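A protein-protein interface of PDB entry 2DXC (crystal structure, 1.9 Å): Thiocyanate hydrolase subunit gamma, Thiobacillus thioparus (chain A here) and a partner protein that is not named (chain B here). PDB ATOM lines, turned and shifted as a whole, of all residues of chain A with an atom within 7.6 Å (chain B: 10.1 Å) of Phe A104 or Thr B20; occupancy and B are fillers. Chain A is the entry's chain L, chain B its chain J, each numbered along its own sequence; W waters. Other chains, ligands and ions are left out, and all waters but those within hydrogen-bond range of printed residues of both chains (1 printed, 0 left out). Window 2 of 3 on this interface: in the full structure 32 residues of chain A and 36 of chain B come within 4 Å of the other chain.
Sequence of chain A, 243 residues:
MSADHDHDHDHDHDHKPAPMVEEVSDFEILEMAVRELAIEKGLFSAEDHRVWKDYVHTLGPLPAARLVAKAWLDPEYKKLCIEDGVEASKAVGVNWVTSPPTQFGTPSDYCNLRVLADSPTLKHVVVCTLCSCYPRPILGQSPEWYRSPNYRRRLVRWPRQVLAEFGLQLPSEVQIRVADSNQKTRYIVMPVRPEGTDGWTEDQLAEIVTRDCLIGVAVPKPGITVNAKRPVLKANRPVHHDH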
ATOM      1  N   TRP A  52      29.206 -33.766  24.348  1.00  0.00           N
ATOM      2  CA  TRP A  52      29.414 -32.542  25.109  1.00  0.00           C
ATOM      3  C   TRP A  52      30.881 -32.205  25.319  1.00  0.00           C
ATOM      4  O   TRP A  52      31.277 -31.047  25.175  1.00  0.00           O
ATOM      5  CB  TRP A  52      28.699 -32.590  26.461  1.00  0.00           C
ATOM      6  CG  TRP A  52      28.422 -31.202  26.925  1.00  0.00           C
ATOM      7  CD1 TRP A  52      29.261 -30.385  27.626  1.00  0.00           C
ATOM      8  CD2 TRP A  52      27.305 -30.393  26.543  1.00  0.00           C
ATOM      9  NE1 TRP A  52      28.741 -29.113  27.694  1.00  0.00           N
ATOM     10  CE2 TRP A  52      27.538 -29.093  27.038  1.00  0.00           C
ATOM     11  CE3 TRP A  52      26.130 -30.644  25.823  1.00  0.00           C
ATOM     12  CZ2 TRP A  52      26.637 -28.040  26.834  1.00  0.00           C
ATOM     13  CZ3 TRP A  52      25.235 -29.598  25.619  1.00  0.00           C
ATOM     14  CH2 TRP A  52      25.496 -28.311  26.125  1.00  0.00           C
ATOM     15  N   TRP A  96      24.345 -18.545  19.511  1.00  0.00           N
ATOM     16  CA  TRP A  96      24.049 -18.960  20.875  1.00  0.00           C
ATOM     17  C   TRP A  96      22.922 -19.971  21.014  1.00  0.00           C
ATOM     18  O   TRP A  96      22.881 -20.731  21.982  1.00  0.00           O
ATOM     19  CB  TRP A  96      23.794 -17.729  21.747  1.00  0.00           C
ATOM     20  CG  TRP A  96      25.073 -17.006  22.054  1.00  0.00           C
ATOM     21  CD1 TRP A  96      25.920 -16.412  21.156  1.00  0.00           C
ATOM     22  CD2 TRP A  96      25.699 -16.888  23.335  1.00  0.00           C
ATOM     23  NE1 TRP A  96      27.039 -15.937  21.803  1.00  0.00           N
ATOM     24  CE2 TRP A  96      26.929 -16.216  23.139  1.00  0.00           C
ATOM     25  CE3 TRP A  96      25.343 -17.287  24.630  1.00  0.00           C
ATOM     26  CZ2 TRP A  96      27.804 -15.935  24.196  1.00  0.00           C
ATOM     27  CZ3 TRP A  96      26.213 -17.006  25.679  1.00  0.00           C
ATOM     28  CH2 TRP A  96      27.429 -16.336  25.454  1.00  0.00           C
ATOM     29  N   VAL A  97      22.017 -20.003  20.047  1.00  0.00           N
ATOM     30  CA  VAL A  97      20.920 -20.955  20.108  1.00  0.00           C
ATOM     31  C   VAL A  97      21.260 -22.278  19.421  1.00  0.00           C
ATOM     32  O   VAL A  97      21.125 -23.347  20.018  1.00  0.00           O
ATOM     33  CB  VAL A  97      19.642 -20.384  19.452  1.00  0.00           C
ATOM     34  CG1 VAL A  97      18.542 -21.453  19.430  1.00  0.00           C
ATOM     35  CG2 VAL A  97      19.167 -19.150  20.217  1.00  0.00           C
ATOM     36  N   THR A  98      21.730 -22.195  18.179  1.00  0.00           N
ATOM     37  CA  THR A  98      22.027 -23.384  17.384  1.00  0.00           C
ATOM     38  C   THR A  98      23.439 -23.981  17.363  1.00  0.00           C
ATOM     39  O   THR A  98      23.618 -25.093  16.870  1.00  0.00           O
ATOM     40  CB  THR A  98      21.600 -23.152  15.921  1.00  0.00           C
ATOM     41  OG1 THR A  98      22.335 -22.047  15.379  1.00  0.00           O
ATOM     42  CG2 THR A  98      20.120 -22.841  15.851  1.00  0.00           C
ATOM     43  N   SER A  99      24.444 -23.277  17.872  1.00  0.00           N
ATOM     44  CA  SER A  99      25.793 -23.848  17.866  1.00  0.00           C
ATOM     45  C   SER A  99      25.953 -24.970  18.899  1.00  0.00           C
ATOM     46  O   SER A  99      26.622 -25.968  18.635  1.00  0.00           O
ATOM     47  CB  SER A  99      26.846 -22.761  18.094  1.00  0.00           C
ATOM     48  OG  SER A  99      26.946 -21.907  16.966  1.00  0.00           O
ATOM     49  N   PRO A 100      25.351 -24.816  20.096  1.00  0.00           N
ATOM     50  CA  PRO A 100      25.459 -25.860  21.125  1.00  0.00           C
ATOM     51  C   PRO A 100      24.678 -27.119  20.718  1.00  0.00           C
ATOM     52  O   PRO A 100      23.668 -27.035  20.017  1.00  0.00           O
ATOM     53  CB  PRO A 100      24.859 -25.190  22.361  1.00  0.00           C
ATOM     54  CG  PRO A 100      25.151 -23.734  22.136  1.00  0.00           C
ATOM     55  CD  PRO A 100      24.801 -23.578  20.677  1.00  0.00           C
ATOM     56  N   PRO A 101      25.128 -28.299  21.171  1.00  0.00           N
ATOM     57  CA  PRO A 101      24.476 -29.578  20.853  1.00  0.00           C
ATOM     58  C   PRO A 101      22.971 -29.613  21.136  1.00  0.00           C
ATOM     59  O   PRO A 101      22.219 -30.321  20.465  1.00  0.00           O
ATOM     60  CB  PRO A 101      25.242 -30.580  21.718  1.00  0.00           C
ATOM     61  CG  PRO A 101      26.614 -29.974  21.796  1.00  0.00           C
ATOM     62  CD  PRO A 101      26.302 -28.511  22.037  1.00  0.00           C
ATOM     63  N   THR A 102      22.540 -28.844  22.129  1.00  0.00           N
ATOM     64  CA  THR A 102      21.134 -28.789  22.527  1.00  0.00           C
ATOM     65  C   THR A 102      20.189 -28.203  21.483  1.00  0.00           C
ATOM     66  O   THR A 102      19.036 -28.620  21.378  1.00  0.00           O
ATOM     67  CB  THR A 102      20.950 -27.921  23.780  1.00  0.00           C
ATOM     68  OG1 THR A 102      21.343 -26.579  23.468  1.00  0.00           O
ATOM     69  CG2 THR A 102      21.791 -28.439  24.935  1.00  0.00           C
ATOM     70  N   GLN A 103      20.683 -27.221  20.738  1.00  0.00           N
ATOM     71  CA  GLN A 103      19.896 -26.505  19.743  1.00  0.00           C
ATOM     72  C   GLN A 103      18.940 -25.537  20.431  1.00  0.00           C
ATOM     73  O   GLN A 103      17.958 -25.080  19.840  1.00  0.00           O
ATOM     74  CB  GLN A 103      19.113 -27.450  18.829  1.00  0.00           C
ATOM     75  CG  GLN A 103      19.947 -28.015  17.698  1.00  0.00           C
ATOM     76  CD  GLN A 103      21.112 -27.105  17.319  1.00  0.00           C
ATOM     77  OE1 GLN A 103      20.911 -25.944  16.956  1.00  0.00           O
ATOM     78  NE2 GLN A 103      22.337 -27.628  17.408  1.00  0.00           N
ATOM     79  N   PHE A 104      19.215 -25.253  21.700  1.00  0.00           N
ATOM     80  CA  PHE A 104      18.430 -24.283  22.450  1.00  0.00           C
ATOM     81  C   PHE A 104      19.362 -23.562  23.418  1.00  0.00           C
ATOM     82  O   PHE A 104      18.958 -23.115  24.489  1.00  0.00           O
ATOM     83  CB  PHE A 104      17.218 -24.935  23.164  1.00  0.00           C
ATOM     84  CG  PHE A 104      17.555 -26.063  24.115  1.00  0.00           C
ATOM     85  CD1 PHE A 104      18.138 -25.811  25.353  1.00  0.00           C
ATOM     86  CD2 PHE A 104      17.207 -27.375  23.801  1.00  0.00           C
ATOM     87  CE1 PHE A 104      18.364 -26.846  26.266  1.00  0.00           C
ATOM     88  CE2 PHE A 104      17.428 -28.418  24.704  1.00  0.00           C
ATOM     89  CZ  PHE A 104      18.008 -28.150  25.942  1.00  0.00           C
ATOM     90  N   GLY A 105      20.619 -23.429  22.987  1.00  0.00           N
ATOM     91  CA  GLY A 105      21.644 -22.786  23.792  1.00  0.00           C
ATOM     92  C   GLY A 105      22.127 -23.763  24.845  1.00  0.00           C
ATOM     93  O   GLY A 105      21.434 -24.743  25.128  1.00  0.00           O
ATOM     94  N   THR A 106      23.308 -23.535  25.416  1.00  0.00           N
ATOM     95  CA  THR A 106      23.783 -24.449  26.451  1.00  0.00           C
ATOM     96  C   THR A 106      22.826 -24.273  27.629  1.00  0.00           C
ATOM     97  O   THR A 106      22.264 -23.193  27.829  1.00  0.00           O
ATOM     98  CB  THR A 106      25.213 -24.124  26.929  1.00  0.00           C
ATOM     99  OG1 THR A 106      25.229 -22.823  27.526  1.00  0.00           O
ATOM    100  CG2 THR A 106      26.202 -24.175  25.763  1.00  0.00           C
ATOM    101  N   PRO A 107      22.617 -25.334  28.416  1.00  0.00           N
ATOM    102  CA  PRO A 107      21.706 -25.219  29.558  1.00  0.00           C
ATOM    103  C   PRO A 107      22.138 -24.172  30.585  1.00  0.00           C
ATOM    104  O   PRO A 107      21.298 -23.478  31.163  1.00  0.00           O
ATOM    105  CB  PRO A 107      21.713 -26.630  30.149  1.00  0.00           C
ATOM    106  CG  PRO A 107      21.997 -27.497  28.952  1.00  0.00           C
ATOM    107  CD  PRO A 107      23.081 -26.722  28.247  1.00  0.00           C
ATOM    108  N   SER A 108      23.445 -24.047  30.793  1.00  0.00           N
ATOM    109  CA  SER A 108      23.964 -23.122  31.798  1.00  0.00           C
ATOM    110  C   SER A 108      24.388 -21.724  31.349  1.00  0.00           C
ATOM    111  O   SER A 108      24.500 -20.823  32.180  1.00  0.00           O
ATOM    112  CB  SER A 108      25.128 -23.782  32.542  1.00  0.00           C
ATOM    113  OG  SER A 108      24.712 -24.993  33.157  1.00  0.00           O
ATOM    114  N   TYR A 110      22.826 -20.098  28.589  1.00  0.00           N
ATOM    115  CA  TYR A 110      21.645 -19.471  27.995  1.00  0.00           C
ATOM    116  C   TYR A 110      21.903 -18.773  26.661  1.00  0.00           C
ATOM    117  O   TYR A 110      22.951 -18.960  26.047  1.00  0.00           O
ATOM    118  CB  TYR A 110      21.010 -18.489  28.987  1.00  0.00           C
ATOM    119  CG  TYR A 110      20.660 -19.140  30.307  1.00  0.00           C
ATOM    120  CD1 TYR A 110      21.458 -18.949  31.433  1.00  0.00           C
ATOM    121  CD2 TYR A 110      19.562 -19.998  30.416  1.00  0.00           C
ATOM    122  CE1 TYR A 110      21.179 -19.594  32.633  1.00  0.00           C
ATOM    123  CE2 TYR A 110      19.274 -20.652  31.615  1.00  0.00           C
ATOM    124  CZ  TYR A 110      20.088 -20.442  32.718  1.00  0.00           C
ATOM    125  OH  TYR A 110      19.814 -21.076  33.908  1.00  0.00           O
ATOM    126  N   CYS A 111      20.944 -17.964  26.217  1.00  0.00           N
ATOM    127  CA  CYS A 111      21.073 -17.293  24.928  1.00  0.00           C
ATOM    128  C   CYS A 111      20.889 -15.778  24.958  1.00  0.00           C
ATOM    129  O   CYS A 111      20.140 -15.227  24.154  1.00  0.00           O
ATOM    130  CB  CYS A 111      20.069 -17.899  23.948  1.00  0.00           C
ATOM    131  SG  CYS A 111      20.052 -19.712  23.960  1.00  0.00           S
ATOM    132  N   ARG B  12      10.850 -35.081  31.294  1.00  0.00           N
ATOM    133  CA  ARG B  12      12.184 -34.718  30.843  1.00  0.00           C
ATOM    134  C   ARG B  12      12.216 -34.199  29.406  1.00  0.00           C
ATOM    135  O   ARG B  12      13.292 -33.955  28.860  1.00  0.00           O
ATOM    136  CB  ARG B  12      13.121 -35.922  30.984  1.00  0.00           C
ATOM    137  CG  ARG B  12      12.970 -36.642  32.317  1.00  0.00           C
ATOM    138  CD  ARG B  12      14.286 -37.205  32.812  1.00  0.00           C
ATOM    139  NE  ARG B  12      14.883 -38.161  31.884  1.00  0.00           N
ATOM    140  CZ  ARG B  12      14.505 -39.429  31.752  1.00  0.00           C
ATOM    141  NH1 ARG B  12      13.518 -39.914  32.493  1.00  0.00           N
ATOM    142  NH2 ARG B  12      15.124 -40.215  30.880  1.00  0.00           N
ATOM    143  N   THR B  13      11.045 -34.017  28.798  1.00  0.00           N
ATOM    144  CA  THR B  13      10.981 -33.532  27.418  1.00  0.00           C
ATOM    145  C   THR B  13      10.446 -32.108  27.294  1.00  0.00           C
ATOM    146  O   THR B  13      10.689 -31.436  26.294  1.00  0.00           O
ATOM    147  CB  THR B  13      10.090 -34.437  26.537  1.00  0.00           C
ATOM    148  OG1 THR B  13       8.733 -34.363  26.994  1.00  0.00           O
ATOM    149  CG2 THR B  13      10.559 -35.880  26.599  1.00  0.00           C
ATOM    150  N   HIS B  14       9.719 -31.652  28.308  1.00  0.00           N
ATOM    151  CA  HIS B  14       9.133 -30.317  28.284  1.00  0.00           C
ATOM    152  C   HIS B  14      10.069 -29.182  27.864  1.00  0.00           C
ATOM    153  O   HIS B  14       9.774 -28.444  26.925  1.00  0.00           O
ATOM    154  CB  HIS B  14       8.534 -29.977  29.650  1.00  0.00           C
ATOM    155  CG  HIS B  14       8.125 -28.543  29.783  1.00  0.00           C
ATOM    156  ND1 HIS B  14       7.021 -28.021  29.142  1.00  0.00           N
ATOM    157  CD2 HIS B  14       8.710 -27.507  30.427  1.00  0.00           C
ATOM    158  CE1 HIS B  14       6.947 -26.725  29.385  1.00  0.00           C
ATOM    159  NE2 HIS B  14       7.961 -26.388  30.162  1.00  0.00           N
ATOM    160  N   HIS B  15      11.190 -29.032  28.560  1.00  0.00           N
ATOM    161  CA  HIS B  15      12.114 -27.947  28.252  1.00  0.00           C
ATOM    162  C   HIS B  15      12.637 -27.968  26.815  1.00  0.00           C
ATOM    163  O   HIS B  15      12.627 -26.944  26.134  1.00  0.00           O
ATOM    164  CB  HIS B  15      13.289 -27.951  29.233  1.00  0.00           C
ATOM    165  CG  HIS B  15      14.157 -26.737  29.130  1.00  0.00           C
ATOM    166  ND1 HIS B  15      13.702 -25.472  29.431  1.00  0.00           N
ATOM    167  CD2 HIS B  15      15.442 -26.590  28.726  1.00  0.00           C
ATOM    168  CE1 HIS B  15      14.668 -24.597  29.216  1.00  0.00           C
ATOM    169  NE2 HIS B  15      15.733 -25.248  28.787  1.00  0.00           N
ATOM    170  N   ALA B  16      13.090 -29.129  26.357  1.00  0.00           N
ATOM    171  CA  ALA B  16      13.610 -29.261  25.002  1.00  0.00           C
ATOM    172  C   ALA B  16      12.536 -28.963  23.959  1.00  0.00           C
ATOM    173  O   ALA B  16      12.787 -28.248  22.987  1.00  0.00           O
ATOM    174  CB  ALA B  16      14.165 -30.664  24.790  1.00  0.00           C
ATOM    175  N   LYS B  17      11.343 -29.514  24.152  1.00  0.00           N
ATOM    176  CA  LYS B  17      10.254 -29.288  23.209  1.00  0.00           C
ATOM    177  C   LYS B  17       9.909 -27.808  23.130  1.00  0.00           C
ATOM    178  O   LYS B  17       9.566 -27.290  22.068  1.00  0.00           O
ATOM    179  CB  LYS B  17       9.006 -30.078  23.625  1.00  0.00           C
ATOM    180  CG  LYS B  17       9.129 -31.587  23.450  1.00  0.00           C
ATOM    181  CD  LYS B  17       7.840 -32.300  23.845  1.00  0.00           C
ATOM    182  CE  LYS B  17       7.940 -33.804  23.608  1.00  0.00           C
ATOM    183  NZ  LYS B  17       6.716 -34.525  24.064  1.00  0.00           N
ATOM    184  N   MET B  18      10.016 -27.126  24.262  1.00  0.00           N
ATOM    185  CA  MET B  18       9.687 -25.710  24.328  1.00  0.00           C
ATOM    186  C   MET B  18      10.757 -24.762  23.789  1.00  0.00           C
ATOM    187  O   MET B  18      10.436 -23.779  23.123  1.00  0.00           O
ATOM    188  CB  MET B  18       9.367 -25.330  25.779  1.00  0.00           C
ATOM    189  CG  MET B  18       9.086 -23.854  25.989  1.00  0.00           C
ATOM    190  SD  MET B  18       8.848 -23.431  27.731  1.00  0.00           S
ATOM    191  CE  MET B  18      10.562 -23.249  28.257  1.00  0.00           C
ATOM    192  N   ALA B  19      12.025 -25.054  24.063  1.00  0.00           N
ATOM    193  CA  ALA B  19      13.105 -24.158  23.650  1.00  0.00           C
ATOM    194  C   ALA B  19      13.908 -24.506  22.397  1.00  0.00           C
ATOM    195  O   ALA B  19      14.623 -23.649  21.874  1.00  0.00           O
ATOM    196  CB  ALA B  19      14.063 -23.953  24.821  1.00  0.00           C
ATOM    197  N   THR B  20      13.807 -25.739  21.912  1.00  0.00           N
ATOM    198  CA  THR B  20      14.576 -26.131  20.734  1.00  0.00           C
ATOM    199  C   THR B  20      14.321 -25.224  19.537  1.00  0.00           C
ATOM    200  O   THR B  20      13.175 -25.012  19.136  1.00  0.00           O
ATOM    201  CB  THR B  20      14.289 -27.593  20.323  1.00  0.00           C
ATOM    202  OG1 THR B  20      14.756 -28.473  21.352  1.00  0.00           O
ATOM    203  CG2 THR B  20      15.005 -27.936  19.015  1.00  0.00           C
ATOM    204  N   GLY B  21      15.403 -24.682  18.985  1.00  0.00           N
ATOM    205  CA  GLY B  21      15.294 -23.811  17.832  1.00  0.00           C
ATOM    206  C   GLY B  21      14.860 -22.402  18.172  1.00  0.00           C
ATOM    207  O   GLY B  21      14.734 -21.564  17.283  1.00  0.00           O
ATOM    208  N   ILE B  22      14.630 -22.138  19.455  1.00  0.00           N
ATOM    209  CA  ILE B  22      14.203 -20.814  19.900  1.00  0.00           C
ATOM    210  C   ILE B  22      15.198 -20.245  20.904  1.00  0.00           C
ATOM    211  O   ILE B  22      15.661 -19.115  20.764  1.00  0.00           O
ATOM    212  CB  ILE B  22      12.804 -20.861  20.569  1.00  0.00           C
ATOM    213  CG1 ILE B  22      11.765 -21.382  19.576  1.00  0.00           C
ATOM    214  CG2 ILE B  22      12.400 -19.476  21.054  1.00  0.00           C
ATOM    215  CD1 ILE B  22      11.408 -22.829  19.787  1.00  0.00           C
ATOM    216  N   GLY B  23      15.519 -21.037  21.920  1.00  0.00           N
ATOM    217  CA  GLY B  23      16.455 -20.592  22.933  1.00  0.00           C
ATOM    218  C   GLY B  23      15.798 -20.214  24.249  1.00  0.00           C
ATOM    219  O   GLY B  23      14.573 -20.133  24.352  1.00  0.00           O
ATOM    220  N   ASP B  24      16.640 -19.985  25.251  1.00  0.00           N
ATOM    221  CA  ASP B  24      16.228 -19.608  26.606  1.00  0.00           C
ATOM    222  C   ASP B  24      17.048 -18.343  26.874  1.00  0.00           C
ATOM    223  O   ASP B  24      18.273 -18.369  26.777  1.00  0.00           O
ATOM    224  CB  ASP B  24      16.620 -20.732  27.571  1.00  0.00           C
ATOM    225  CG  ASP B  24      16.179 -20.476  29.003  1.00  0.00           C
ATOM    226  OD1 ASP B  24      15.738 -19.349  29.315  1.00  0.00           O
ATOM    227  OD2 ASP B  24      16.290 -21.421  29.822  1.00  0.00           O
ATOM    228  N   PRO B  25      16.407 -17.244  27.313  1.00  0.00           N
ATOM    229  CA  PRO B  25      14.985 -16.988  27.574  1.00  0.00           C
ATOM    230  C   PRO B  25      14.064 -16.640  26.408  1.00  0.00           C
ATOM    231  O   PRO B  25      12.922 -16.239  26.635  1.00  0.00           O
ATOM    232  CB  PRO B  25      15.051 -15.848  28.581  1.00  0.00           C
ATOM    233  CG  PRO B  25      16.155 -15.013  28.013  1.00  0.00           C
ATOM    234  CD  PRO B  25      17.211 -16.045  27.614  1.00  0.00           C
ATOM    235  N   GLN B  26      14.535 -16.781  25.171  1.00  0.00           N
ATOM    236  CA  GLN B  26      13.692 -16.451  24.025  1.00  0.00           C
ATOM    237  C   GLN B  26      12.342 -17.174  24.044  1.00  0.00           C
ATOM    238  O   GLN B  26      11.337 -16.617  23.613  1.00  0.00           O
ATOM    239  CB  GLN B  26      14.410 -16.764  22.699  1.00  0.00           C
ATOM    240  CG  GLN B  26      15.482 -15.751  22.298  1.00  0.00           C
ATOM    241  CD  GLN B  26      16.845 -16.074  22.880  1.00  0.00           C
ATOM    242  OE1 GLN B  26      16.950 -16.762  23.892  1.00  0.00           O
ATOM    243  NE2 GLN B  26      17.899 -15.568  22.243  1.00  0.00           N
ATOM    244  N   CYS B  27      12.316 -18.402  24.553  1.00  0.00           N
ATOM    245  CA  CYS B  27      11.077 -19.179  24.593  1.00  0.00           C
ATOM    246  C   CYS B  27       9.998 -18.624  25.526  1.00  0.00           C
ATOM    247  O   CYS B  27       8.862 -19.099  25.509  1.00  0.00           O
ATOM    248  CB  CYS B  27      11.383 -20.628  24.979  1.00  0.00           C
ATOM    249  SG  CYS B  27      12.265 -20.812  26.546  1.00  0.00           S
ATOM    250  N   PHE B  28      10.350 -17.622  26.328  1.00  0.00           N
ATOM    251  CA  PHE B  28       9.405 -17.012  27.266  1.00  0.00           C
ATOM    252  C   PHE B  28       8.927 -15.643  26.791  1.00  0.00           C
ATOM    253  O   PHE B  28       8.105 -15.001  27.446  1.00  0.00           O
ATOM    254  CB  PHE B  28      10.058 -16.851  28.641  1.00  0.00           C
ATOM    255  CG  PHE B  28      10.502 -18.143  29.254  1.00  0.00           C
ATOM    256  CD1 PHE B  28       9.570 -19.103  29.638  1.00  0.00           C
ATOM    257  CD2 PHE B  28      11.856 -18.409  29.436  1.00  0.00           C
ATOM    258  CE1 PHE B  28       9.984 -20.312  30.195  1.00  0.00           C
ATOM    259  CE2 PHE B  28      12.279 -19.615  29.993  1.00  0.00           C
ATOM    260  CZ  PHE B  28      11.344 -20.566  30.372  1.00  0.00           C
HETATM  261  O   HOH W   1      17.506 -13.534  24.671  1.00  0.00           O
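Among the printed residues, merely in contact across the chains: Phe A104 with Ala B19, Tyr A110 with Asp B24, Val A97 with Ile B22, Phe A104 with Thr B20, Gln A103 with Thr B20, Phe A104 with His B15, Cys A111 with Gly B23, Phe A104 with Gly B23, Phe A104 with Ala B16, Val A97 with Gly B23 and Phe A104 with Asp B24.
The backbone NH (N) of Gly B21 lies within hydrogen-bond range of the backbone carbonyl oxygen (O) of Gln A103 (2.7 Å).
NE2 of Gln B26 is in hydrogen-bond range of O of Cys A111 (3.0 Å).
O of Asp B24 lies within hydrogen-bond range of N of Cys A111, 2.8 Å away.
Of chain B, only His B15 (3.8 Å), Ala B16 (3.9 Å), Ala B19 (3.2 Å), Thr B20 (3.6 Å), Gly B23 (3.9 Å) and Asp B24 (3.97 Å) come within 4 Å of Phe A104.
Of chain A, only Gln A103 and Phe A104 come within 4 Å of Thr B20.
Gln A103 touches just these residues of chain B: Thr B20 and Gly B21.
No residue of chain B comes within 4 Å of Gly A105.
Of chain A, only Phe A104 (3.2 Å) comes within 4 Å of Ala B19.
Printed residues of chain B within 4 Å of Val A97: Ile B22 (3.5 Å) and Gly B23 (3.9 Å).
Of the printed residues of chain A, Gly B23 touches Val A97 (3.9 Å), Phe A104 (3.9 Å) and Cys A111 (3.8 Å).
Of the printed residues of chain A, Gln B26 touches Cys A111.
Pro A101 touches none of the printed residues of chain B.
Met B18 touches none of the printed residues of chain A.
Water W1 lies within hydrogen-bond range of O of Cys A111 (3.2 Å) and NE2 of Gln B26 (3.2 Å).
The backbone NH (N) of Phe A104 lies within hydrogen-bond range of the backbone carbonyl oxygen (O) of Val A97 (3.2 Å).
The backbone carbonyl oxygen (O) of Trp A96 is in hydrogen-bond range of the side-chain sulfur (SG) of Cys A111, 3.6 Å away.
O of Val A97 lies within hydrogen-bond range of N of Gly A105 (3.0 Å).
O of Thr A98 sits close to OE1 of Gln A103 (2.8 Å).
The backbone NH (N) of Phe A104 is in hydrogen-bond range of the side-chain hydroxyl (OG1) of Thr A102 (3.1 Å).
The side-chain hydroxyl (OG1) of Thr B20 sits at hydrogen-bond distance from the backbone carbonyl oxygen (O) of Ala B16.
Hydrophobic or aromatic side chains of chain B that line the printed part of chain A: His B15, Ala B16 and Ala B19.
Printed residues of chain A that touch a printed residue of chain B: Val A97, Gln A103, Phe A104, Tyr A110 and Cys A111.
Hydrophobic or aromatic side chains of chain A within 4 Å of the printed part of chain B: Val A97, Phe A104 and Tyr A110.
Among the printed residues, 14 pairs touch across the chains.
Among the printed residues, no Asp or Glu carboxylate lies within 4 Å of a Lys or Arg side-chain nitrogen of the other chain.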
